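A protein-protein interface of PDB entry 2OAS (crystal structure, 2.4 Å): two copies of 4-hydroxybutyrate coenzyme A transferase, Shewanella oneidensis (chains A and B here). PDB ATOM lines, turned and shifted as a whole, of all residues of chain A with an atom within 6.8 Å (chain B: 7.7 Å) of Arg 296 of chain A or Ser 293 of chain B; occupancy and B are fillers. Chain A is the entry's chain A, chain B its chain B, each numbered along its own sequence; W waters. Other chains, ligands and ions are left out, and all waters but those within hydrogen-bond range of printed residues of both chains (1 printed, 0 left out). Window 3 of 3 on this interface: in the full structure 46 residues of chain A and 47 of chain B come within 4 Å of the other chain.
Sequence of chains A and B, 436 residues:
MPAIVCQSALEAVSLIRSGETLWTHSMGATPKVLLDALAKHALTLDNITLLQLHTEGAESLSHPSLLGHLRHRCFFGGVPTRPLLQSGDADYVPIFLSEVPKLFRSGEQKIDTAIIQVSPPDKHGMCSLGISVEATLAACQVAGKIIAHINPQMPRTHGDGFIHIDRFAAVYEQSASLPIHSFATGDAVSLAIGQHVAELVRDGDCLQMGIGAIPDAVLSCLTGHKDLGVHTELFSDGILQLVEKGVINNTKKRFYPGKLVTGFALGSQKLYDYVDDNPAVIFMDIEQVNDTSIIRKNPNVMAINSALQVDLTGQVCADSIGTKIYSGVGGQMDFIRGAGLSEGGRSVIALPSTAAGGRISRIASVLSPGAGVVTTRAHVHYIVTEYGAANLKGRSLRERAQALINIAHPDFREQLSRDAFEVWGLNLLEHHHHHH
The side-chain carboxylate of Asp 291 of chain A lies within salt-bridge range of the guanidinium group of Arg 296 of chain B (3.5 Å).
The guanidinium group (NE) of Arg 337 of chain A lies within salt-bridge range of the side-chain carboxylate (OE2) of Glu 99 of chain B (3.1 Å).
The guanidinium group (NH1) of Arg 337 of chain A is in salt-bridge range of the side-chain carboxylate (OD2) of Asp 334 of chain B (2.9 Å).
NH1 of Arg 296 of chain A lies within salt-bridge range of OD2 of Asp 291 of chain B (3.4 Å).
The side-chain carboxylate (OD1) of Asp 291 of chain B is in hydrogen-bond range of the backbone NH (N) of Ser 293 of chain B (2.9 Å).
OD1 of Asp 291 of chain A is in hydrogen-bond range of N of Ser 293 of chain A, at 2.8 Å.
Among the printed residues, pairs that only touch across the chains: Ser 293 of chain A with Arg 296 of chain B (3.9 Å), Arg 296 of chain A with Ser 293 of chain B (3.9 Å) and Leu 341 of chain A with Glu 99 of chain B (3.6 Å).
Ser 293 of chain B touches just one residue of chain A: Arg 296.
Of the printed residues of chain B, Leu 341 of chain A touches Glu 99 (3.6 Å).
Of the printed residues of chain A, Asp 334 of chain B touches Arg 337.
Of the printed residues of chain B, Ser 293 of chain A touches Arg 296 (3.9 Å).
Printed residues of chain A within 4 Å of Asp 291 of chain B: Arg 296 (3.4 Å).
Ala 339 of chain A touches none of the printed residues of chain B.
Lys 297 of chain A touches none of the printed residues of chain B.
The nearest residue of chain B that does not touch Arg 296 of chain A is Glu 287 of chain B (6.1 Å).
The nearest residue of chain A that does not touch Ser 293 of chain B is Ser 293 of chain A (4.4 Å).
The nearest printed residue of chain B that does not touch Arg 337 of chain A is Thr 292 of chain B (5.1 Å).
Along chain B the printed residues that touch a printed residue of chain A span positions 99 to 334.
Of the 17 printed residues of chain A, 5 touch a printed residue of chain B.
Among the printed residues, 7 pairs touch across the chains.
Among the printed residues, Asp or Glu carboxylates within 4 Å of a Lys or Arg side-chain nitrogen of the other chain: Asp 291 of chain A with Arg 296 of chain B, Arg 296 of chain A with Asp 291 of chain B, Arg 337 of chain A with Glu 99 of chain B and Arg 337 of chain A with Asp 334 of chain B.
Asp 291 of chain A touches Arg 296 of chain B, and with the chains exchanged Arg 296 of chain A touches Asp 291 of chain B.
Ser 293 of chain A touches Arg 296 of chain B, and with the chains exchanged Arg 296 of chain A touches Ser 293 of chain B.
Positions printed for both chains: 291, 292, 293, 294, 295, 296, 297, 298, 338 and 341.
Water W1 lies within hydrogen-bond range of NH2 of Arg 337 of chain A (3.2 Å) and N of Thr 292 of chain B (3.2 Å).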
ATOM      1  N   ASP A 291     -19.523   5.516  17.406  1.00  0.00           N
ATOM      2  CA  ASP A 291     -18.481   6.434  16.955  1.00  0.00           C
ATOM      3  C   ASP A 291     -18.634   6.648  15.445  1.00  0.00           C
ATOM      4  O   ASP A 291     -18.422   5.724  14.650  1.00  0.00           O
ATOM      5  CB  ASP A 291     -17.096   5.863  17.257  1.00  0.00           C
ATOM      6  CG  ASP A 291     -15.999   6.904  17.120  1.00  0.00           C
ATOM      7  OD1 ASP A 291     -16.014   7.631  16.108  1.00  0.00           O
ATOM      8  OD2 ASP A 291     -15.124   7.001  18.020  1.00  0.00           O
ATOM      9  N   THR A 292     -19.002   7.871  15.055  1.00  0.00           N
ATOM     10  CA  THR A 292     -19.209   8.202  13.652  1.00  0.00           C
ATOM     11  C   THR A 292     -18.005   7.804  12.805  1.00  0.00           C
ATOM     12  O   THR A 292     -18.142   7.418  11.645  1.00  0.00           O
ATOM     13  CB  THR A 292     -19.503   9.717  13.469  1.00  0.00           C
ATOM     14  OG1 THR A 292     -18.355  10.494  13.857  1.00  0.00           O
ATOM     15  CG2 THR A 292     -20.697  10.126  14.326  1.00  0.00           C
ATOM     16  N   SER A 293     -16.822   7.892  13.391  1.00  0.00           N
ATOM     17  CA  SER A 293     -15.610   7.531  12.688  1.00  0.00           C
ATOM     18  C   SER A 293     -15.606   6.039  12.327  1.00  0.00           C
ATOM     19  O   SER A 293     -14.992   5.623  11.334  1.00  0.00           O
ATOM     20  CB  SER A 293     -14.396   7.883  13.554  1.00  0.00           C
ATOM     21  OG  SER A 293     -13.213   7.300  13.044  1.00  0.00           O
ATOM     22  N   ILE A 294     -16.292   5.229  13.125  1.00  0.00           N
ATOM     23  CA  ILE A 294     -16.366   3.787  12.859  1.00  0.00           C
ATOM     24  C   ILE A 294     -17.562   3.439  11.977  1.00  0.00           C
ATOM     25  O   ILE A 294     -17.441   2.657  11.036  1.00  0.00           O
ATOM     26  CB  ILE A 294     -16.458   2.987  14.167  1.00  0.00           C
ATOM     27  CG1 ILE A 294     -15.131   3.085  14.904  1.00  0.00           C
ATOM     28  CG2 ILE A 294     -16.807   1.537  13.879  1.00  0.00           C
ATOM     29  CD1 ILE A 294     -15.157   2.423  16.244  1.00  0.00           C
ATOM     30  N   ILE A 295     -18.709   4.035  12.286  1.00  0.00           N
ATOM     31  CA  ILE A 295     -19.930   3.790  11.536  1.00  0.00           C
ATOM     32  C   ILE A 295     -19.774   4.037  10.031  1.00  0.00           C
ATOM     33  O   ILE A 295     -20.270   3.258   9.205  1.00  0.00           O
ATOM     34  CB  ILE A 295     -21.068   4.683  12.059  1.00  0.00           C
ATOM     35  CG1 ILE A 295     -21.198   4.521  13.572  1.00  0.00           C
ATOM     36  CG2 ILE A 295     -22.373   4.331  11.364  1.00  0.00           C
ATOM     37  CD1 ILE A 295     -22.246   5.411  14.194  1.00  0.00           C
ATOM     38  N   ARG A 296     -19.094   5.130   9.685  1.00  0.00           N
ATOM     39  CA  ARG A 296     -18.842   5.510   8.288  1.00  0.00           C
ATOM     40  C   ARG A 296     -17.993   4.474   7.543  1.00  0.00           C
ATOM     41  O   ARG A 296     -17.942   4.485   6.313  1.00  0.00           O
ATOM     42  CB  ARG A 296     -18.125   6.864   8.224  1.00  0.00           C
ATOM     43  CG  ARG A 296     -16.643   6.792   8.597  1.00  0.00           C
ATOM     44  CD  ARG A 296     -15.950   8.163   8.526  1.00  0.00           C
ATOM     45  NE  ARG A 296     -16.117   8.805   7.224  1.00  0.00           N
ATOM     46  CZ  ARG A 296     -15.621   9.998   6.909  1.00  0.00           C
ATOM     47  NH1 ARG A 296     -14.920  10.683   7.802  1.00  0.00           N
ATOM     48  NH2 ARG A 296     -15.842  10.511   5.704  1.00  0.00           N
ATOM     49  N   LYS A 297     -17.325   3.584   8.276  1.00  0.00           N
ATOM     50  CA  LYS A 297     -16.483   2.570   7.631  1.00  0.00           C
ATOM     51  C   LYS A 297     -17.291   1.554   6.821  1.00  0.00           C
ATOM     52  O   LYS A 297     -16.768   0.935   5.892  1.00  0.00           O
ATOM     53  CB  LYS A 297     -15.607   1.835   8.662  1.00  0.00           C
ATOM     54  CG  LYS A 297     -14.521   2.699   9.290  1.00  0.00           C
ATOM     55  CD  LYS A 297     -13.691   1.929  10.295  1.00  0.00           C
ATOM     56  CE  LYS A 297     -12.591   2.813  10.891  1.00  0.00           C
ATOM     57  NZ  LYS A 297     -11.748   2.067  11.873  1.00  0.00           N
ATOM     58  N   ASN A 298     -18.561   1.383   7.172  1.00  0.00           N
ATOM     59  CA  ASN A 298     -19.418   0.453   6.449  1.00  0.00           C
ATOM     60  C   ASN A 298     -20.203   1.172   5.370  1.00  0.00           C
ATOM     61  O   ASN A 298     -20.879   2.173   5.640  1.00  0.00           O
ATOM     62  CB  ASN A 298     -20.416  -0.225   7.379  1.00  0.00           C
ATOM     63  CG  ASN A 298     -19.780  -1.264   8.243  1.00  0.00           C
ATOM     64  OD1 ASN A 298     -18.952  -2.046   7.775  1.00  0.00           O
ATOM     65  ND2 ASN A 298     -20.162  -1.299   9.508  1.00  0.00           N
ATOM     66  N   PRO A 299     -20.136   0.663   4.130  1.00  0.00           N
ATOM     67  CA  PRO A 299     -20.850   1.262   2.993  1.00  0.00           C
ATOM     68  C   PRO A 299     -22.351   1.036   3.052  1.00  0.00           C
ATOM     69  O   PRO A 299     -22.824   0.054   3.620  1.00  0.00           O
ATOM     70  CB  PRO A 299     -20.207   0.575   1.788  1.00  0.00           C
ATOM     71  CG  PRO A 299     -19.822  -0.770   2.338  1.00  0.00           C
ATOM     72  CD  PRO A 299     -19.254  -0.431   3.683  1.00  0.00           C
ATOM     73  N   VAL A 301     -24.737   2.507   4.766  1.00  0.00           N
ATOM     74  CA  VAL A 301     -25.344   2.505   6.085  1.00  0.00           C
ATOM     75  C   VAL A 301     -26.780   3.032   5.966  1.00  0.00           C
ATOM     76  O   VAL A 301     -27.040   3.965   5.210  1.00  0.00           O
ATOM     77  CB  VAL A 301     -24.547   3.412   7.065  1.00  0.00           C
ATOM     78  CG1 VAL A 301     -25.399   3.775   8.272  1.00  0.00           C
ATOM     79  CG2 VAL A 301     -23.282   2.691   7.512  1.00  0.00           C
ATOM     80  N   ARG A 337     -25.171  11.155  11.081  1.00  0.00           N
ATOM     81  CA  ARG A 337     -24.019  11.790  10.456  1.00  0.00           C
ATOM     82  C   ARG A 337     -23.158  10.720   9.780  1.00  0.00           C
ATOM     83  O   ARG A 337     -22.787  10.862   8.616  1.00  0.00           O
ATOM     84  CB  ARG A 337     -23.166  12.546  11.486  1.00  0.00           C
ATOM     85  CG  ARG A 337     -22.006  13.364  10.856  1.00  0.00           C
ATOM     86  CD  ARG A 337     -22.529  14.390   9.856  1.00  0.00           C
ATOM     87  NE  ARG A 337     -21.525  15.312   9.322  1.00  0.00           N
ATOM     88  CZ  ARG A 337     -20.792  16.160  10.049  1.00  0.00           C
ATOM     89  NH1 ARG A 337     -20.935  16.205  11.367  1.00  0.00           N
ATOM     90  NH2 ARG A 337     -19.935  16.984   9.449  1.00  0.00           N
ATOM     91  N   GLY A 338     -22.857   9.656  10.532  1.00  0.00           N
ATOM     92  CA  GLY A 338     -22.052   8.570  10.020  1.00  0.00           C
ATOM     93  C   GLY A 338     -22.700   8.000   8.784  1.00  0.00           C
ATOM     94  O   GLY A 338     -22.028   7.593   7.832  1.00  0.00           O
ATOM     95  N   ALA A 339     -24.025   7.979   8.792  1.00  0.00           N
ATOM     96  CA  ALA A 339     -24.768   7.479   7.657  1.00  0.00           C
ATOM     97  C   ALA A 339     -24.542   8.392   6.451  1.00  0.00           C
ATOM     98  O   ALA A 339     -24.472   7.912   5.324  1.00  0.00           O
ATOM     99  CB  ALA A 339     -26.250   7.397   7.999  1.00  0.00           C
ATOM    100  N   GLY A 340     -24.417   9.698   6.682  1.00  0.00           N
ATOM    101  CA  GLY A 340     -24.182  10.626   5.581  1.00  0.00           C
ATOM    102  C   GLY A 340     -22.764  10.531   5.036  1.00  0.00           C
ATOM    103  O   GLY A 340     -22.520  10.743   3.846  1.00  0.00           O
ATOM    104  N   LEU A 341     -21.827  10.216   5.923  1.00  0.00           N
ATOM    105  CA  LEU A 341     -20.425  10.072   5.576  1.00  0.00           C
ATOM    106  C   LEU A 341     -20.159   8.740   4.875  1.00  0.00           C
ATOM    107  O   LEU A 341     -19.237   8.632   4.067  1.00  0.00           O
ATOM    108  CB  LEU A 341     -19.567  10.173   6.840  1.00  0.00           C
ATOM    109  CG  LEU A 341     -19.606  11.546   7.516  1.00  0.00           C
ATOM    110  CD1 LEU A 341     -18.980  11.472   8.899  1.00  0.00           C
ATOM    111  CD2 LEU A 341     -18.889  12.556   6.644  1.00  0.00           C
ATOM    112  N   SER A 342     -20.974   7.735   5.182  1.00  0.00           N
ATOM    113  CA  SER A 342     -20.839   6.405   4.574  1.00  0.00           C
ATOM    114  C   SER A 342     -21.140   6.411   3.076  1.00  0.00           C
ATOM    115  O   SER A 342     -21.989   7.169   2.601  1.00  0.00           O
ATOM    116  CB  SER A 342     -21.777   5.409   5.267  1.00  0.00           C
ATOM    117  OG  SER A 342     -21.938   4.239   4.479  1.00  0.00           O
ATOM    118  N   GLU A 343     -20.456   5.553   2.332  1.00  0.00           N
ATOM    119  CA  GLU A 343     -20.665   5.498   0.887  1.00  0.00           C
ATOM    120  C   GLU A 343     -22.063   5.014   0.530  1.00  0.00           C
ATOM    121  O   GLU A 343     -22.405   3.852   0.739  1.00  0.00           O
ATOM    122  CB  GLU A 343     -19.623   4.587   0.228  1.00  0.00           C
ATOM    123  CG  GLU A 343     -18.178   4.924   0.581  1.00  0.00           C
ATOM    124  CD  GLU A 343     -17.175   3.984  -0.092  1.00  0.00           C
ATOM    125  OE1 GLU A 343     -17.247   2.750   0.151  1.00  0.00           O
ATOM    126  OE2 GLU A 343     -16.321   4.481  -0.865  1.00  0.00           O
ATOM    127  N   GLU B  99     -19.680  19.035   4.214  1.00  0.00           N
ATOM    128  CA  GLU B  99     -20.594  18.200   3.438  1.00  0.00           C
ATOM    129  C   GLU B  99     -20.833  18.774   2.056  1.00  0.00           C
ATOM    130  O   GLU B  99     -21.378  18.097   1.191  1.00  0.00           O
ATOM    131  CB  GLU B  99     -21.961  18.073   4.124  1.00  0.00           C
ATOM    132  CG  GLU B  99     -21.969  17.487   5.529  1.00  0.00           C
ATOM    133  CD  GLU B  99     -21.609  16.015   5.566  1.00  0.00           C
ATOM    134  OE1 GLU B  99     -22.204  15.223   4.791  1.00  0.00           O
ATOM    135  OE2 GLU B  99     -20.734  15.648   6.382  1.00  0.00           O
ATOM    136  N   PHE B 255      -1.033  15.804  12.473  1.00  0.00           N
ATOM    137  CA  PHE B 255      -1.528  15.837  11.107  1.00  0.00           C
ATOM    138  C   PHE B 255      -0.969  17.090  10.469  1.00  0.00           C
ATOM    139  O   PHE B 255      -1.394  18.198  10.783  1.00  0.00           O
ATOM    140  CB  PHE B 255      -3.055  15.854  11.102  1.00  0.00           C
ATOM    141  CG  PHE B 255      -3.656  15.964   9.734  1.00  0.00           C
ATOM    142  CD1 PHE B 255      -3.933  17.209   9.180  1.00  0.00           C
ATOM    143  CD2 PHE B 255      -3.955  14.822   8.997  1.00  0.00           C
ATOM    144  CE1 PHE B 255      -4.504  17.313   7.908  1.00  0.00           C
ATOM    145  CE2 PHE B 255      -4.521  14.913   7.733  1.00  0.00           C
ATOM    146  CZ  PHE B 255      -4.796  16.162   7.185  1.00  0.00           C
ATOM    147  N   GLU B 287     -13.466  19.513   2.954  1.00  0.00           N
ATOM    148  CA  GLU B 287     -13.944  18.159   3.215  1.00  0.00           C
ATOM    149  C   GLU B 287     -12.992  17.434   4.157  1.00  0.00           C
ATOM    150  O   GLU B 287     -13.382  16.481   4.826  1.00  0.00           O
ATOM    151  CB  GLU B 287     -14.085  17.377   1.916  1.00  0.00           C
ATOM    152  CG  GLU B 287     -14.615  15.970   2.113  1.00  0.00           C
ATOM    153  CD  GLU B 287     -14.988  15.298   0.806  1.00  0.00           C
ATOM    154  OE1 GLU B 287     -15.285  14.088   0.821  1.00  0.00           O
ATOM    155  OE2 GLU B 287     -14.990  15.989  -0.239  1.00  0.00           O
ATOM    156  N   GLN B 288     -11.749  17.909   4.208  1.00  0.00           N
ATOM    157  CA  GLN B 288     -10.720  17.340   5.068  1.00  0.00           C
ATOM    158  C   GLN B 288     -10.441  18.206   6.302  1.00  0.00           C
ATOM    159  O   GLN B 288     -10.497  17.722   7.432  1.00  0.00           O
ATOM    160  CB  GLN B 288      -9.408  17.156   4.296  1.00  0.00           C
ATOM    161  CG  GLN B 288      -9.218  15.804   3.641  1.00  0.00           C
ATOM    162  CD  GLN B 288     -10.273  15.498   2.597  1.00  0.00           C
ATOM    163  OE1 GLN B 288     -11.251  14.795   2.870  1.00  0.00           O
ATOM    164  NE2 GLN B 288     -10.084  16.027   1.394  1.00  0.00           N
ATOM    165  N   ASN B 290     -12.198  20.331   7.726  1.00  0.00           N
ATOM    166  CA  ASN B 290     -13.364  20.369   8.602  1.00  0.00           C
ATOM    167  C   ASN B 290     -13.956  18.995   8.884  1.00  0.00           C
ATOM    168  O   ASN B 290     -15.148  18.868   9.206  1.00  0.00           O
ATOM    169  CB  ASN B 290     -14.442  21.275   8.013  1.00  0.00           C
ATOM    170  CG  ASN B 290     -14.162  22.726   8.256  1.00  0.00           C
ATOM    171  OD1 ASN B 290     -13.049  23.188   8.048  1.00  0.00           O
ATOM    172  ND2 ASN B 290     -15.175  23.461   8.699  1.00  0.00           N
ATOM    173  N   ASP B 291     -13.116  17.969   8.751  1.00  0.00           N
ATOM    174  CA  ASP B 291     -13.527  16.592   9.006  1.00  0.00           C
ATOM    175  C   ASP B 291     -13.142  16.215  10.442  1.00  0.00           C
ATOM    176  O   ASP B 291     -11.963  16.111  10.769  1.00  0.00           O
ATOM    177  CB  ASP B 291     -12.846  15.640   8.020  1.00  0.00           C
ATOM    178  CG  ASP B 291     -13.475  14.255   8.025  1.00  0.00           C
ATOM    179  OD1 ASP B 291     -13.735  13.737   9.132  1.00  0.00           O
ATOM    180  OD2 ASP B 291     -13.706  13.684   6.930  1.00  0.00           O
ATOM    181  N   THR B 292     -14.149  16.015  11.291  1.00  0.00           N
ATOM    182  CA  THR B 292     -13.920  15.674  12.687  1.00  0.00           C
ATOM    183  C   THR B 292     -12.960  14.505  12.831  1.00  0.00           C
ATOM    184  O   THR B 292     -12.170  14.446  13.773  1.00  0.00           O
ATOM    185  CB  THR B 292     -15.256  15.360  13.414  1.00  0.00           C
ATOM    186  OG1 THR B 292     -15.846  14.183  12.856  1.00  0.00           O
ATOM    187  CG2 THR B 292     -16.231  16.523  13.248  1.00  0.00           C
ATOM    188  N   SER B 293     -13.024  13.576  11.890  1.00  0.00           N
ATOM    189  CA  SER B 293     -12.142  12.415  11.907  1.00  0.00           C
ATOM    190  C   SER B 293     -10.664  12.833  11.791  1.00  0.00           C
ATOM    191  O   SER B 293      -9.781  12.165  12.325  1.00  0.00           O
ATOM    192  CB  SER B 293     -12.526  11.474  10.763  1.00  0.00           C
ATOM    193  OG  SER B 293     -11.528  10.495  10.553  1.00  0.00           O
ATOM    194  N   ILE B 294     -10.406  13.947  11.107  1.00  0.00           N
ATOM    195  CA  ILE B 294      -9.049  14.447  10.944  1.00  0.00           C
ATOM    196  C   ILE B 294      -8.653  15.392  12.072  1.00  0.00           C
ATOM    197  O   ILE B 294      -7.541  15.312  12.590  1.00  0.00           O
ATOM    198  CB  ILE B 294      -8.888  15.189   9.608  1.00  0.00           C
ATOM    199  CG1 ILE B 294      -8.986  14.195   8.458  1.00  0.00           C
ATOM    200  CG2 ILE B 294      -7.552  15.925   9.562  1.00  0.00           C
ATOM    201  CD1 ILE B 294      -8.917  14.840   7.115  1.00  0.00           C
ATOM    202  N   ILE B 295      -9.563  16.286  12.442  1.00  0.00           N
ATOM    203  CA  ILE B 295      -9.309  17.256  13.504  1.00  0.00           C
ATOM    204  C   ILE B 295      -8.895  16.607  14.829  1.00  0.00           C
ATOM    205  O   ILE B 295      -7.994  17.098  15.511  1.00  0.00           O
ATOM    206  CB  ILE B 295     -10.552  18.114  13.761  1.00  0.00           C
ATOM    207  CG1 ILE B 295     -11.034  18.729  12.451  1.00  0.00           C
ATOM    208  CG2 ILE B 295     -10.221  19.195  14.774  1.00  0.00           C
ATOM    209  CD1 ILE B 295     -12.305  19.541  12.598  1.00  0.00           C
ATOM    210  N   ARG B 296      -9.571  15.513  15.184  1.00  0.00           N
ATOM    211  CA  ARG B 296      -9.289  14.767  16.412  1.00  0.00           C
ATOM    212  C   ARG B 296      -7.884  14.154  16.418  1.00  0.00           C
ATOM    213  O   ARG B 296      -7.395  13.747  17.466  1.00  0.00           O
ATOM    214  CB  ARG B 296     -10.309  13.636  16.589  1.00  0.00           C
ATOM    215  CG  ARG B 296     -10.060  12.443  15.656  1.00  0.00           C
ATOM    216  CD  ARG B 296     -11.076  11.320  15.850  1.00  0.00           C
ATOM    217  NE  ARG B 296     -11.160  10.868  17.240  1.00  0.00           N
ATOM    218  CZ  ARG B 296     -11.992   9.922  17.673  1.00  0.00           C
ATOM    219  NH1 ARG B 296     -12.815   9.312  16.830  1.00  0.00           N
ATOM    220  NH2 ARG B 296     -12.014   9.596  18.960  1.00  0.00           N
ATOM    221  N   LYS B 297      -7.245  14.078  15.252  1.00  0.00           N
ATOM    222  CA  LYS B 297      -5.900  13.499  15.176  1.00  0.00           C
ATOM    223  C   LYS B 297      -4.855  14.338  15.907  1.00  0.00           C
ATOM    224  O   LYS B 297      -3.837  13.809  16.345  1.00  0.00           O
ATOM    225  CB  LYS B 297      -5.476  13.286  13.718  1.00  0.00           C
ATOM    226  CG  LYS B 297      -6.250  12.187  12.993  1.00  0.00           C
ATOM    227  CD  LYS B 297      -5.783  11.996  11.560  1.00  0.00           C
ATOM    228  CE  LYS B 297      -6.554  10.864  10.888  1.00  0.00           C
ATOM    229  NZ  LYS B 297      -6.125  10.639   9.467  1.00  0.00           N
ATOM    230  N   ASN B 298      -5.110  15.636  16.042  1.00  0.00           N
ATOM    231  CA  ASN B 298      -4.177  16.517  16.740  1.00  0.00           C
ATOM    232  C   ASN B 298      -4.555  16.655  18.206  1.00  0.00           C
ATOM    233  O   ASN B 298      -5.698  16.971  18.538  1.00  0.00           O
ATOM    234  CB  ASN B 298      -4.168  17.909  16.122  1.00  0.00           C
ATOM    235  CG  ASN B 298      -3.458  17.950  14.808  1.00  0.00           C
ATOM    236  OD1 ASN B 298      -2.403  17.330  14.649  1.00  0.00           O
ATOM    237  ND2 ASN B 298      -4.014  18.691  13.851  1.00  0.00           N
ATOM    238  N   ASP B 334     -18.445  20.746  13.872  1.00  0.00           N
ATOM    239  CA  ASP B 334     -17.441  19.726  13.603  1.00  0.00           C
ATOM    240  C   ASP B 334     -16.170  19.991  14.410  1.00  0.00           C
ATOM    241  O   ASP B 334     -15.546  19.058  14.910  1.00  0.00           O
ATOM    242  CB  ASP B 334     -17.106  19.701  12.110  1.00  0.00           C
ATOM    243  CG  ASP B 334     -18.173  19.006  11.276  1.00  0.00           C
ATOM    244  OD1 ASP B 334     -18.119  19.141  10.035  1.00  0.00           O
ATOM    245  OD2 ASP B 334     -19.053  18.324  11.849  1.00  0.00           O
ATOM    246  N   GLY B 338     -14.760  17.542  17.263  1.00  0.00           N
ATOM    247  CA  GLY B 338     -13.412  17.050  17.072  1.00  0.00           C
ATOM    248  C   GLY B 338     -12.565  17.463  18.247  1.00  0.00           C
ATOM    249  O   GLY B 338     -11.699  16.718  18.708  1.00  0.00           O
ATOM    250  N   LEU B 341     -13.171  15.089  21.068  1.00  0.00           N
ATOM    251  CA  LEU B 341     -12.585  13.788  20.774  1.00  0.00           C
ATOM    252  C   LEU B 341     -11.062  13.826  20.872  1.00  0.00           C
ATOM    253  O   LEU B 341     -10.434  12.808  21.147  1.00  0.00           O
ATOM    254  CB  LEU B 341     -12.994  13.352  19.364  1.00  0.00           C
ATOM    255  CG  LEU B 341     -14.493  13.105  19.174  1.00  0.00           C
ATOM    256  CD1 LEU B 341     -14.843  12.989  17.703  1.00  0.00           C
ATOM    257  CD2 LEU B 341     -14.875  11.846  19.937  1.00  0.00           C
HETATM  258  O   HOH W   1     -17.085  15.725  10.062  1.00  0.00           O
